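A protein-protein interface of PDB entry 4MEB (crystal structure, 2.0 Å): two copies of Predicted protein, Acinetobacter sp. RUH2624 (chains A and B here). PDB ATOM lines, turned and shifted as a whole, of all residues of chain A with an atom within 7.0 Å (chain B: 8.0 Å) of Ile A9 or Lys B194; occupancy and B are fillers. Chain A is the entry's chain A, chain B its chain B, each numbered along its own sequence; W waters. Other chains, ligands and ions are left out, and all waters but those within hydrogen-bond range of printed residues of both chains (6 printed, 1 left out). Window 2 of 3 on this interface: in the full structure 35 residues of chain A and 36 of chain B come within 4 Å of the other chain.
The side-chain hydroxyl of Tyr A206 lies close to the backbone NH of Gly B189 (3.4 Å). The side-chain hydroxyl (OH) of Tyr B185 sits at hydrogen-bond distance from the side-chain amide nitrogen (NE2) of Gln A195 (3.0 Å). The backbone carbonyl oxygen of Ile A9 is in hydrogen-bond range of the side-chain amino group of Lys B194 (2.9 Å). OG of Ser A8 sits at hydrogen-bond distance from OD1 of Asp B190 (2.7 Å). OD1 of Asn B198 is in hydrogen-bond range of ND2 of Asn A198. The side-chain hydroxyl (OG) of Ser A8 is in hydrogen-bond range of the side-chain amino group (NZ) of Lys B194 (2.8 Å).
OD2 of Asp B190 lies within salt-bridge range of NZ of Lys B194 (3.8 Å). OD1 of Asp A199 sits at hydrogen-bond distance from N of Leu A202. The side-chain amide oxygen of Gln B195 is in hydrogen-bond range of the side-chain hydroxyl of Tyr B185 (2.8 Å).
Among the printed residues, pairs that only touch across the chains: Tyr A206 with Phe B188, Gln A195 with Ile B196, Gln A195 with Gln B195, Phe A203 with Gln B195, Tyr A206 with Ile B191, Leu A202 with Lys B194 and Phe A203 with Ile B191.
Of chain B, only Lys B194 comes within 4 Å of Ile A9. Of the printed residues of chain A, Asp B190 touches Ser A8. Of the printed residues of chain A, Lys B194 touches Ser A8, Ile A9 and Leu A202. Of the printed residues of chain A, Ile B196 touches Gln A195 (3.5 Å). Of the printed residues of chain A, Asn B198 touches Asn A198. The nearest residue of chain B that does not touch Ile A9 is Asp B190 (6.4 Å). The nearest printed residue of chain A that does not touch Lys B194 is Asp A10 (4.7 Å).
Of the 18 printed residues of chain B, 9 touch a printed residue of chain A. Printed residues of chain B that touch a printed residue of chain A: Tyr B185, Phe B188, Gly B189, Asp B190, Ile B191, Lys B194, Gln B195, Ile B196 and Asn B198. Hydrophobic or aromatic side chains of chain B within 4 Å of the printed part of chain A: Tyr B185, Phe B188, Ile B191 and Ile B196. Of the 19 printed residues of chain A, 7 touch a printed residue of chain B. Printed residues of chain A that touch a printed residue of chain B: Ser A8, Ile A9, Gln A195, Asn A198, Leu A202, Phe A203 and Tyr A206. Hydrophobic or aromatic side chains of chain A within 4 Å of the printed part of chain B: Leu A202, Phe A203 and Tyr A206. Among the printed residues, no Asp or Glu carboxylate lies within 4 Å of a Lys or Arg side-chain nitrogen of the other chain.
Gln B195 touches its own counterpart, Gln A195. Asn B198 touches its own counterpart, Asn A198.
Water W5 lies within hydrogen-bond range of O of Asp A199 (2.7 Å), NE2 of Gln B195 (2.9 Å) and O of Gln A195 (3.2 Å). Water W6 bridges N of Ser A8 (3.0 Å) and OD2 of Asp B190 (3.2 Å). Water W4 bridges NZ of Lys B194 and O of Ile A9. Water W1 lies within hydrogen-bond range of the side-chain amide nitrogen (ND2) of Asn B198 (3.3 Å) and the side-chain amide oxygen (OD1) of Asn A198 (3.3 Å). Water W2 lies within hydrogen-bond range of the side-chain amide nitrogen of Asn A198 (3.3 Å) and the side-chain amide oxygen of Asn B198 (3.3 Å).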
ATOM      1  N   LYS A   7     -22.418   7.414  10.813  1.00  0.00           N
ATOM      2  CA  LYS A   7     -23.717   6.771  10.648  1.00  0.00           C
ATOM      3  C   LYS A   7     -24.516   7.451   9.547  1.00  0.00           C
ATOM      4  O   LYS A   7     -24.385   8.656   9.334  1.00  0.00           O
ATOM      5  CB  LYS A   7     -24.501   6.806  11.960  1.00  0.00           C
ATOM      6  CG  LYS A   7     -23.767   6.127  13.105  1.00  0.00           C
ATOM      7  CD  LYS A   7     -24.605   6.066  14.367  1.00  0.00           C
ATOM      8  CE  LYS A   7     -23.912   5.204  15.418  1.00  0.00           C
ATOM      9  NZ  LYS A   7     -23.428   3.917  14.832  1.00  0.00           N
ATOM     10  N   SER A   8     -25.334   6.680   8.834  1.00  0.00           N
ATOM     11  CA  SER A   8     -26.230   7.278   7.848  1.00  0.00           C
ATOM     12  C   SER A   8     -27.457   7.788   8.583  1.00  0.00           C
ATOM     13  O   SER A   8     -27.729   7.357   9.707  1.00  0.00           O
ATOM     14  CB  SER A   8     -26.630   6.259   6.782  1.00  0.00           C
ATOM     15  OG  SER A   8     -27.138   5.088   7.388  1.00  0.00           O
ATOM     16  N   ILE A   9     -28.197   8.701   7.964  1.00  0.00           N
ATOM     17  CA  ILE A   9     -29.392   9.244   8.601  1.00  0.00           C
ATOM     18  C   ILE A   9     -30.546   8.246   8.513  1.00  0.00           C
ATOM     19  O   ILE A   9     -30.465   7.266   7.770  1.00  0.00           O
ATOM     20  CB  ILE A   9     -29.838  10.538   7.915  1.00  0.00           C
ATOM     21  CG1 ILE A   9     -30.190  10.241   6.446  1.00  0.00           C
ATOM     22  CG2 ILE A   9     -28.745  11.590   8.015  1.00  0.00           C
ATOM     23  CD1 ILE A   9     -30.781  11.408   5.703  1.00  0.00           C
ATOM     24  N   ASP A  10     -31.611   8.489   9.278  1.00  0.00           N
ATOM     25  CA  ASP A  10     -32.828   7.687   9.180  1.00  0.00           C
ATOM     26  C   ASP A  10     -34.046   8.553   8.873  1.00  0.00           C
ATOM     27  O   ASP A  10     -35.181   8.146   9.097  1.00  0.00           O
ATOM     28  CB  ASP A  10     -33.066   6.864  10.454  1.00  0.00           C
ATOM     29  CG  ASP A  10     -33.118   7.714  11.719  1.00  0.00           C
ATOM     30  OD1 ASP A  10     -33.459   8.918  11.655  1.00  0.00           O
ATOM     31  OD2 ASP A  10     -32.816   7.158  12.796  1.00  0.00           O
ATOM     32  N   THR A  11     -33.800   9.755   8.370  1.00  0.00           N
ATOM     33  CA  THR A  11     -34.873  10.665   8.008  1.00  0.00           C
ATOM     34  C   THR A  11     -35.743  10.056   6.915  1.00  0.00           C
ATOM     35  O   THR A  11     -35.228   9.561   5.911  1.00  0.00           O
ATOM     36  CB  THR A  11     -34.295  11.979   7.484  1.00  0.00           C
ATOM     37  OG1 THR A  11     -33.227  12.396   8.341  1.00  0.00           O
ATOM     38  CG2 THR A  11     -35.372  13.056   7.430  1.00  0.00           C
ATOM     39  N   PRO A  12     -37.070  10.081   7.107  1.00  0.00           N
ATOM     40  CA  PRO A  12     -37.934   9.610   6.020  1.00  0.00           C
ATOM     41  C   PRO A  12     -37.762  10.473   4.765  1.00  0.00           C
ATOM     42  O   PRO A  12     -37.673  11.693   4.873  1.00  0.00           O
ATOM     43  CB  PRO A  12     -39.356   9.768   6.596  1.00  0.00           C
ATOM     44  CG  PRO A  12     -39.158   9.728   8.112  1.00  0.00           C
ATOM     45  CD  PRO A  12     -37.822  10.405   8.335  1.00  0.00           C
ATOM     46  N   SER A  16     -37.456  14.636   4.003  1.00  0.00           N
ATOM     47  CA  SER A  16     -36.358  15.271   3.280  1.00  0.00           C
ATOM     48  C   SER A  16     -36.901  16.103   2.123  1.00  0.00           C
ATOM     49  O   SER A  16     -36.380  17.170   1.830  1.00  0.00           O
ATOM     50  CB  SER A  16     -35.350  14.236   2.767  1.00  0.00           C
ATOM     51  OG  SER A  16     -34.746  13.535   3.852  1.00  0.00           O
ATOM     52  N   GLN A 195     -31.379   4.836  -7.543  1.00  0.00           N
ATOM     53  CA  GLN A 195     -31.281   4.518  -6.129  1.00  0.00           C
ATOM     54  C   GLN A 195     -31.177   5.796  -5.309  1.00  0.00           C
ATOM     55  O   GLN A 195     -31.812   5.929  -4.263  1.00  0.00           O
ATOM     56  CB  GLN A 195     -30.074   3.611  -5.879  1.00  0.00           C
ATOM     57  CG  GLN A 195     -30.263   2.194  -6.404  1.00  0.00           C
ATOM     58  CD  GLN A 195     -29.240   1.228  -5.861  1.00  0.00           C
ATOM     59  OE1 GLN A 195     -29.579   0.102  -5.468  1.00  0.00           O
ATOM     60  NE2 GLN A 195     -27.985   1.654  -5.827  1.00  0.00           N
ATOM     61  N   ASN A 198     -34.307   7.915  -4.965  1.00  0.00           N
ATOM     62  CA  ASN A 198     -35.261   7.395  -3.980  1.00  0.00           C
ATOM     63  C   ASN A 198     -35.067   8.045  -2.622  1.00  0.00           C
ATOM     64  O   ASN A 198     -36.022   8.227  -1.874  1.00  0.00           O
ATOM     65  CB  ASN A 198     -35.159   5.872  -3.840  1.00  0.00           C
ATOM     66  CG  ASN A 198     -36.040   5.322  -2.710  1.00  0.00           C
ATOM     67  OD1 ASN A 198     -35.561   5.047  -1.605  1.00  0.00           O
ATOM     68  ND2 ASN A 198     -37.328   5.157  -2.991  1.00  0.00           N
ATOM     69  N   ASP A 199     -33.828   8.408  -2.316  1.00  0.00           N
ATOM     70  CA  ASP A 199     -33.514   9.054  -1.045  1.00  0.00           C
ATOM     71  C   ASP A 199     -32.181   9.794  -1.163  1.00  0.00           C
ATOM     72  O   ASP A 199     -31.152   9.298  -0.710  1.00  0.00           O
ATOM     73  CB  ASP A 199     -33.472   8.006   0.072  1.00  0.00           C
ATOM     74  CG  ASP A 199     -33.453   8.623   1.461  1.00  0.00           C
ATOM     75  OD1 ASP A 199     -33.251   9.852   1.585  1.00  0.00           O
ATOM     76  OD2 ASP A 199     -33.621   7.866   2.433  1.00  0.00           O
ATOM     77  N   PRO A 200     -32.194  10.976  -1.813  1.00  0.00           N
ATOM     78  CA  PRO A 200     -30.973  11.766  -2.043  1.00  0.00           C
ATOM     79  C   PRO A 200     -30.355  12.216  -0.733  1.00  0.00           C
ATOM     80  O   PRO A 200     -29.141  12.236  -0.612  1.00  0.00           O
ATOM     81  CB  PRO A 200     -31.481  12.996  -2.819  1.00  0.00           C
ATOM     82  CG  PRO A 200     -32.823  12.586  -3.367  1.00  0.00           C
ATOM     83  CD  PRO A 200     -33.393  11.619  -2.383  1.00  0.00           C
ATOM     84  N   ASN A 201     -31.188  12.564   0.246  1.00  0.00           N
ATOM     85  CA  ASN A 201     -30.674  13.007   1.533  1.00  0.00           C
ATOM     86  C   ASN A 201     -29.844  11.900   2.201  1.00  0.00           C
ATOM     87  O   ASN A 201     -28.794  12.180   2.775  1.00  0.00           O
ATOM     88  CB  ASN A 201     -31.811  13.492   2.444  1.00  0.00           C
ATOM     89  CG  ASN A 201     -31.327  14.403   3.564  1.00  0.00           C
ATOM     90  OD1 ASN A 201     -30.183  14.854   3.566  1.00  0.00           O
ATOM     91  ND2 ASN A 201     -32.209  14.692   4.517  1.00  0.00           N
ATOM     92  N   LEU A 202     -30.306  10.651   2.102  1.00  0.00           N
ATOM     93  CA  LEU A 202     -29.577   9.524   2.681  1.00  0.00           C
ATOM     94  C   LEU A 202     -28.198   9.375   2.047  1.00  0.00           C
ATOM     95  O   LEU A 202     -27.195   9.374   2.751  1.00  0.00           O
ATOM     96  CB  LEU A 202     -30.362   8.210   2.553  1.00  0.00           C
ATOM     97  CG  LEU A 202     -29.614   6.904   2.871  1.00  0.00           C
ATOM     98  CD1 LEU A 202     -29.261   6.823   4.330  1.00  0.00           C
ATOM     99  CD2 LEU A 202     -30.443   5.689   2.454  1.00  0.00           C
ATOM    100  N   PHE A 203     -28.145   9.234   0.723  1.00  0.00           N
ATOM    101  CA  PHE A 203     -26.860   9.056   0.051  1.00  0.00           C
ATOM    102  C   PHE A 203     -25.928  10.265   0.229  1.00  0.00           C
ATOM    103  O   PHE A 203     -24.765  10.114   0.605  1.00  0.00           O
ATOM    104  CB  PHE A 203     -27.034   8.737  -1.441  1.00  0.00           C
ATOM    105  CG  PHE A 203     -25.724   8.595  -2.172  1.00  0.00           C
ATOM    106  CD1 PHE A 203     -25.088   7.363  -2.243  1.00  0.00           C
ATOM    107  CD2 PHE A 203     -25.105   9.694  -2.749  1.00  0.00           C
ATOM    108  CE1 PHE A 203     -23.871   7.227  -2.903  1.00  0.00           C
ATOM    109  CE2 PHE A 203     -23.887   9.564  -3.403  1.00  0.00           C
ATOM    110  CZ  PHE A 203     -23.270   8.327  -3.476  1.00  0.00           C
ATOM    111  N   SER A 205     -25.956  12.930   2.364  1.00  0.00           N
ATOM    112  CA  SER A 205     -25.531  13.282   3.717  1.00  0.00           C
ATOM    113  C   SER A 205     -24.315  12.446   4.084  1.00  0.00           C
ATOM    114  O   SER A 205     -23.339  12.952   4.631  1.00  0.00           O
ATOM    115  CB  SER A 205     -26.657  13.078   4.735  1.00  0.00           C
ATOM    116  OG  SER A 205     -27.695  14.034   4.541  1.00  0.00           O
ATOM    117  N   TYR A 206     -24.359  11.169   3.732  1.00  0.00           N
ATOM    118  CA  TYR A 206     -23.250  10.271   4.031  1.00  0.00           C
ATOM    119  C   TYR A 206     -22.043  10.535   3.124  1.00  0.00           C
ATOM    120  O   TYR A 206     -20.906  10.628   3.597  1.00  0.00           O
ATOM    121  CB  TYR A 206     -23.689   8.818   3.909  1.00  0.00           C
ATOM    122  CG  TYR A 206     -22.633   7.851   4.401  1.00  0.00           C
ATOM    123  CD1 TYR A 206     -22.628   7.403   5.721  1.00  0.00           C
ATOM    124  CD2 TYR A 206     -21.628   7.409   3.553  1.00  0.00           C
ATOM    125  CE1 TYR A 206     -21.658   6.514   6.169  1.00  0.00           C
ATOM    126  CE2 TYR A 206     -20.654   6.533   3.992  1.00  0.00           C
ATOM    127  CZ  TYR A 206     -20.672   6.086   5.293  1.00  0.00           C
ATOM    128  OH  TYR A 206     -19.693   5.216   5.712  1.00  0.00           O
ATOM    129  N   LYS A 209     -20.410  14.157   4.024  1.00  0.00           N
ATOM    130  CA  LYS A 209     -19.673  14.124   5.279  1.00  0.00           C
ATOM    131  C   LYS A 209     -18.413  13.276   5.200  1.00  0.00           C
ATOM    132  O   LYS A 209     -17.389  13.635   5.787  1.00  0.00           O
ATOM    133  CB  LYS A 209     -20.564  13.632   6.419  1.00  0.00           C
ATOM    134  CG  LYS A 209     -21.554  14.666   6.907  1.00  0.00           C
ATOM    135  CD  LYS A 209     -22.262  14.107   8.113  1.00  0.00           C
ATOM    136  CE  LYS A 209     -22.946  15.181   8.898  1.00  0.00           C
ATOM    137  NZ  LYS A 209     -23.477  14.602  10.163  1.00  0.00           N
ATOM    138  N   PRO A 220     -27.901  19.470   9.056  1.00  0.00           N
ATOM    139  CA  PRO A 220     -28.982  19.003   8.175  1.00  0.00           C
ATOM    140  C   PRO A 220     -29.502  20.117   7.262  1.00  0.00           C
ATOM    141  O   PRO A 220     -29.806  19.855   6.098  1.00  0.00           O
ATOM    142  CB  PRO A 220     -30.069  18.564   9.163  1.00  0.00           C
ATOM    143  CG  PRO A 220     -29.300  18.127  10.391  1.00  0.00           C
ATOM    144  CD  PRO A 220     -28.146  19.111  10.472  1.00  0.00           C
ATOM    145  N   LEU A 223     -27.005  20.734   4.524  1.00  0.00           N
ATOM    146  CA  LEU A 223     -27.067  19.559   3.662  1.00  0.00           C
ATOM    147  C   LEU A 223     -28.320  19.581   2.790  1.00  0.00           C
ATOM    148  O   LEU A 223     -28.260  19.220   1.615  1.00  0.00           O
ATOM    149  CB  LEU A 223     -27.008  18.259   4.485  1.00  0.00           C
ATOM    150  CG  LEU A 223     -25.618  17.860   5.000  1.00  0.00           C
ATOM    151  CD1 LEU A 223     -25.701  16.688   5.978  1.00  0.00           C
ATOM    152  CD2 LEU A 223     -24.701  17.497   3.824  1.00  0.00           C
ATOM    153  N   TYR B 185     -18.322   0.032  -3.117  1.00  0.00           N
ATOM    154  CA  TYR B 185     -19.729   0.348  -2.863  1.00  0.00           C
ATOM    155  C   TYR B 185     -20.296  -0.531  -1.757  1.00  0.00           C
ATOM    156  O   TYR B 185     -20.991  -0.035  -0.864  1.00  0.00           O
ATOM    157  CB  TYR B 185     -20.570   0.226  -4.139  1.00  0.00           C
ATOM    158  CG  TYR B 185     -22.070   0.437  -3.951  1.00  0.00           C
ATOM    159  CD1 TYR B 185     -22.572   1.617  -3.402  1.00  0.00           C
ATOM    160  CD2 TYR B 185     -22.982  -0.528  -4.369  1.00  0.00           C
ATOM    161  CE1 TYR B 185     -23.952   1.815  -3.258  1.00  0.00           C
ATOM    162  CE2 TYR B 185     -24.352  -0.341  -4.232  1.00  0.00           C
ATOM    163  CZ  TYR B 185     -24.832   0.825  -3.671  1.00  0.00           C
ATOM    164  OH  TYR B 185     -26.195   1.002  -3.540  1.00  0.00           O
ATOM    165  N   PHE B 188     -19.155   0.581   1.808  1.00  0.00           N
ATOM    166  CA  PHE B 188     -19.329   2.017   2.053  1.00  0.00           C
ATOM    167  C   PHE B 188     -20.456   2.216   3.045  1.00  0.00           C
ATOM    168  O   PHE B 188     -21.608   2.369   2.646  1.00  0.00           O
ATOM    169  CB  PHE B 188     -19.688   2.677   0.722  1.00  0.00           C
ATOM    170  CG  PHE B 188     -19.727   4.185   0.743  1.00  0.00           C
ATOM    171  CD1 PHE B 188     -18.575   4.927   0.949  1.00  0.00           C
ATOM    172  CD2 PHE B 188     -20.911   4.857   0.453  1.00  0.00           C
ATOM    173  CE1 PHE B 188     -18.607   6.325   0.916  1.00  0.00           C
ATOM    174  CE2 PHE B 188     -20.956   6.238   0.406  1.00  0.00           C
ATOM    175  CZ  PHE B 188     -19.795   6.979   0.638  1.00  0.00           C
ATOM    176  N   GLY B 189     -20.136   2.189   4.338  1.00  0.00           N
ATOM    177  CA  GLY B 189     -21.158   2.222   5.380  1.00  0.00           C
ATOM    178  C   GLY B 189     -22.280   1.212   5.171  1.00  0.00           C
ATOM    179  O   GLY B 189     -22.033   0.095   4.710  1.00  0.00           O
ATOM    180  N   ASP B 190     -23.510   1.593   5.511  1.00  0.00           N
ATOM    181  CA  ASP B 190     -24.668   0.739   5.242  1.00  0.00           C
ATOM    182  C   ASP B 190     -25.482   1.231   4.043  1.00  0.00           C
ATOM    183  O   ASP B 190     -26.662   0.882   3.894  1.00  0.00           O
ATOM    184  CB  ASP B 190     -25.558   0.579   6.488  1.00  0.00           C
ATOM    185  CG  ASP B 190     -26.196   1.886   6.936  1.00  0.00           C
ATOM    186  OD1 ASP B 190     -25.808   2.966   6.436  1.00  0.00           O
ATOM    187  OD2 ASP B 190     -27.082   1.833   7.820  1.00  0.00           O
ATOM    188  N   ILE B 191     -24.834   2.023   3.189  1.00  0.00           N
ATOM    189  CA  ILE B 191     -25.501   2.639   2.039  1.00  0.00           C
ATOM    190  C   ILE B 191     -26.020   1.613   1.013  1.00  0.00           C
ATOM    191  O   ILE B 191     -27.149   1.727   0.547  1.00  0.00           O
ATOM    192  CB  ILE B 191     -24.595   3.718   1.374  1.00  0.00           C
ATOM    193  CG1 ILE B 191     -24.229   4.815   2.392  1.00  0.00           C
ATOM    194  CG2 ILE B 191     -25.258   4.321   0.147  1.00  0.00           C
ATOM    195  CD1 ILE B 191     -25.430   5.528   3.018  1.00  0.00           C
ATOM    196  N   ALA B 192     -25.212   0.610   0.667  1.00  0.00           N
ATOM    197  CA  ALA B 192     -25.656  -0.394  -0.307  1.00  0.00           C
ATOM    198  C   ALA B 192     -26.842  -1.163   0.259  1.00  0.00           C
ATOM    199  O   ALA B 192     -27.839  -1.406  -0.434  1.00  0.00           O
ATOM    200  CB  ALA B 192     -24.531  -1.360  -0.669  1.00  0.00           C
ATOM    201  N   GLU B 193     -26.719  -1.540   1.530  1.00  0.00           N
ATOM    202  CA  GLU B 193     -27.783  -2.257   2.224  1.00  0.00           C
ATOM    203  C   GLU B 193     -29.102  -1.488   2.143  1.00  0.00           C
ATOM    204  O   GLU B 193     -30.129  -2.033   1.728  1.00  0.00           O
ATOM    205  CB  GLU B 193     -27.412  -2.501   3.688  1.00  0.00           C
ATOM    206  CG  GLU B 193     -28.575  -3.030   4.521  1.00  0.00           C
ATOM    207  CD  GLU B 193     -28.295  -2.994   6.006  1.00  0.00           C
ATOM    208  OE1 GLU B 193     -27.100  -2.959   6.386  1.00  0.00           O
ATOM    209  OE2 GLU B 193     -29.269  -2.991   6.789  1.00  0.00           O
ATOM    210  N   LYS B 194     -29.066  -0.220   2.535  1.00  0.00           N
ATOM    211  CA  LYS B 194     -30.270   0.601   2.556  1.00  0.00           C
ATOM    212  C   LYS B 194     -30.817   0.864   1.150  1.00  0.00           C
ATOM    213  O   LYS B 194     -32.025   0.791   0.924  1.00  0.00           O
ATOM    214  CB  LYS B 194     -30.010   1.922   3.284  1.00  0.00           C
ATOM    215  CG  LYS B 194     -30.039   1.809   4.806  1.00  0.00           C
ATOM    216  CD  LYS B 194     -29.767   3.162   5.452  1.00  0.00           C
ATOM    217  CE  LYS B 194     -30.042   3.128   6.949  1.00  0.00           C
ATOM    218  NZ  LYS B 194     -29.837   4.482   7.534  1.00  0.00           N
ATOM    219  N   GLN B 195     -29.930   1.162   0.208  1.00  0.00           N
ATOM    220  CA  GLN B 195     -30.367   1.522  -1.132  1.00  0.00           C
ATOM    221  C   GLN B 195     -30.961   0.318  -1.858  1.00  0.00           C
ATOM    222  O   GLN B 195     -32.052   0.394  -2.435  1.00  0.00           O
ATOM    223  CB  GLN B 195     -29.215   2.141  -1.932  1.00  0.00           C
ATOM    224  CG  GLN B 195     -28.912   3.587  -1.531  1.00  0.00           C
ATOM    225  CD  GLN B 195     -27.961   4.269  -2.486  1.00  0.00           C
ATOM    226  OE1 GLN B 195     -27.023   3.653  -3.008  1.00  0.00           O
ATOM    227  NE2 GLN B 195     -28.190   5.553  -2.716  1.00  0.00           N
ATOM    228  N   ILE B 196     -30.248  -0.797  -1.808  1.00  0.00           N
ATOM    229  CA  ILE B 196     -30.700  -2.022  -2.460  1.00  0.00           C
ATOM    230  C   ILE B 196     -31.967  -2.616  -1.812  1.00  0.00           C
ATOM    231  O   ILE B 196     -32.859  -3.104  -2.517  1.00  0.00           O
ATOM    232  CB  ILE B 196     -29.565  -3.054  -2.544  1.00  0.00           C
ATOM    233  CG1 ILE B 196     -28.463  -2.531  -3.473  1.00  0.00           C
ATOM    234  CG2 ILE B 196     -30.096  -4.418  -3.023  1.00  0.00           C
ATOM    235  CD1 ILE B 196     -27.193  -3.367  -3.460  1.00  0.00           C
ATOM    236  N   ALA B 197     -32.073  -2.544  -0.486  1.00  0.00           N
ATOM    237  CA  ALA B 197     -33.277  -3.054   0.184  1.00  0.00           C
ATOM    238  C   ALA B 197     -34.522  -2.310  -0.285  1.00  0.00           C
ATOM    239  O   ALA B 197     -35.615  -2.872  -0.304  1.00  0.00           O
ATOM    240  CB  ALA B 197     -33.146  -2.994   1.710  1.00  0.00           C
ATOM    241  N   ASN B 198     -34.359  -1.050  -0.675  1.00  0.00           N
ATOM    242  CA  ASN B 198     -35.483  -0.297  -1.211  1.00  0.00           C
ATOM    243  C   ASN B 198     -36.038  -0.897  -2.507  1.00  0.00           C
ATOM    244  O   ASN B 198     -37.245  -0.857  -2.746  1.00  0.00           O
ATOM    245  CB  ASN B 198     -35.141   1.185  -1.415  1.00  0.00           C
ATOM    246  CG  ASN B 198     -36.306   1.965  -2.021  1.00  0.00           C
ATOM    247  OD1 ASN B 198     -36.340   2.227  -3.226  1.00  0.00           O
ATOM    248  ND2 ASN B 198     -37.277   2.316  -1.187  1.00  0.00           N
ATOM    249  N   ASP B 199     -35.165  -1.454  -3.338  1.00  0.00           N
ATOM    250  CA  ASP B 199     -35.620  -2.094  -4.578  1.00  0.00           C
ATOM    251  C   ASP B 199     -34.617  -3.160  -5.010  1.00  0.00           C
ATOM    252  O   ASP B 199     -33.792  -2.910  -5.882  1.00  0.00           O
ATOM    253  CB  ASP B 199     -35.787  -1.032  -5.673  1.00  0.00           C
ATOM    254  CG  ASP B 199     -36.591  -1.523  -6.879  1.00  0.00           C
ATOM    255  OD1 ASP B 199     -36.745  -2.749  -7.072  1.00  0.00           O
ATOM    256  OD2 ASP B 199     -37.056  -0.658  -7.656  1.00  0.00           O
ATOM    257  N   PRO B 200     -34.663  -4.348  -4.372  1.00  0.00           N
ATOM    258  CA  PRO B 200     -33.658  -5.384  -4.663  1.00  0.00           C
ATOM    259  C   PRO B 200     -33.728  -5.846  -6.111  1.00  0.00           C
ATOM    260  O   PRO B 200     -32.697  -6.068  -6.743  1.00  0.00           O
ATOM    261  CB  PRO B 200     -34.052  -6.526  -3.721  1.00  0.00           C
ATOM    262  CG  PRO B 200     -34.759  -5.846  -2.595  1.00  0.00           C
ATOM    263  CD  PRO B 200     -35.512  -4.712  -3.222  1.00  0.00           C
ATOM    264  N   ARG B 233     -33.140  -6.336   4.418  1.00  0.00           N
ATOM    265  CA  ARG B 233     -31.977  -5.666   4.992  1.00  0.00           C
ATOM    266  C   ARG B 233     -31.061  -6.650   5.721  1.00  0.00           C
ATOM    267  O   ARG B 233     -29.839  -6.519   5.662  1.00  0.00           O
ATOM    268  CB  ARG B 233     -32.386  -4.556   5.969  1.00  0.00           C
ATOM    269  CG  ARG B 233     -33.294  -3.479   5.415  1.00  0.00           C
ATOM    270  CD  ARG B 233     -32.630  -2.100   5.330  1.00  0.00           C
ATOM    271  NE  ARG B 233     -31.620  -1.797   6.354  1.00  0.00           N
ATOM    272  CZ  ARG B 233     -31.694  -0.791   7.227  1.00  0.00           C
ATOM    273  NH1 ARG B 233     -32.751   0.004   7.253  1.00  0.00           N
ATOM    274  NH2 ARG B 233     -30.712  -0.586   8.095  1.00  0.00           N
ATOM    275  N   LEU B 236     -28.981  -8.502   3.145  1.00  0.00           N
ATOM    276  CA  LEU B 236     -28.046  -7.601   2.485  1.00  0.00           C
ATOM    277  C   LEU B 236     -26.948  -7.184   3.447  1.00  0.00           C
ATOM    278  O   LEU B 236     -25.790  -7.099   3.060  1.00  0.00           O
ATOM    279  CB  LEU B 236     -28.771  -6.380   1.921  1.00  0.00           C
ATOM    280  CG  LEU B 236     -29.654  -6.738   0.726  1.00  0.00           C
ATOM    281  CD1 LEU B 236     -30.666  -5.633   0.480  1.00  0.00           C
ATOM    282  CD2 LEU B 236     -28.788  -6.999  -0.517  1.00  0.00           C
ATOM    283  N   LYS B 237     -27.312  -6.923   4.704  1.00  0.00           N
ATOM    284  CA  LYS B 237     -26.304  -6.617   5.716  1.00  0.00           C
ATOM    285  C   LYS B 237     -25.258  -7.741   5.815  1.00  0.00           C
ATOM    286  O   LYS B 237     -24.055  -7.486   5.820  1.00  0.00           O
ATOM    287  CB  LYS B 237     -26.946  -6.362   7.084  1.00  0.00           C
ATOM    288  CG  LYS B 237     -25.944  -5.871   8.137  1.00  0.00           C
ATOM    289  CD  LYS B 237     -26.607  -5.682   9.498  1.00  0.00           C
ATOM    290  CE  LYS B 237     -25.619  -5.140  10.533  1.00  0.00           C
ATOM    291  NZ  LYS B 237     -26.292  -4.818  11.826  1.00  0.00           N
ATOM    292  N   PHE B 240     -22.986  -7.865   2.653  1.00  0.00           N
ATOM    293  CA  PHE B 240     -22.027  -6.768   2.559  1.00  0.00           C
ATOM    294  C   PHE B 240     -21.009  -6.798   3.707  1.00  0.00           C
ATOM    295  O   PHE B 240     -19.960  -6.141   3.654  1.00  0.00           O
ATOM    296  CB  PHE B 240     -22.772  -5.428   2.411  1.00  0.00           C
ATOM    297  CG  PHE B 240     -23.656  -5.378   1.180  1.00  0.00           C
ATOM    298  CD1 PHE B 240     -23.271  -6.038   0.022  1.00  0.00           C
ATOM    299  CD2 PHE B 240     -24.876  -4.715   1.194  1.00  0.00           C
ATOM    300  CE1 PHE B 240     -24.079  -6.017  -1.118  1.00  0.00           C
ATOM    301  CE2 PHE B 240     -25.690  -4.691   0.072  1.00  0.00           C
ATOM    302  CZ  PHE B 240     -25.291  -5.340  -1.090  1.00  0.00           C
HETATM  303  O   HOH W   1     -37.028   4.405   1.328  1.00  0.00           O
HETATM  304  O   HOH W   2     -38.784   3.260  -5.253  1.00  0.00           O
HETATM  305  O   HOH W   3     -32.365   3.122  -3.285  1.00  0.00           O
HETATM  306  O   HOH W   4     -32.492   5.325   6.017  1.00  0.00           O
HETATM  307  O   HOH W   5     -30.497   6.803  -1.452  1.00  0.00           O
HETATM  308  O   HOH W   6     -25.476   3.820   9.766  1.00  0.00           O
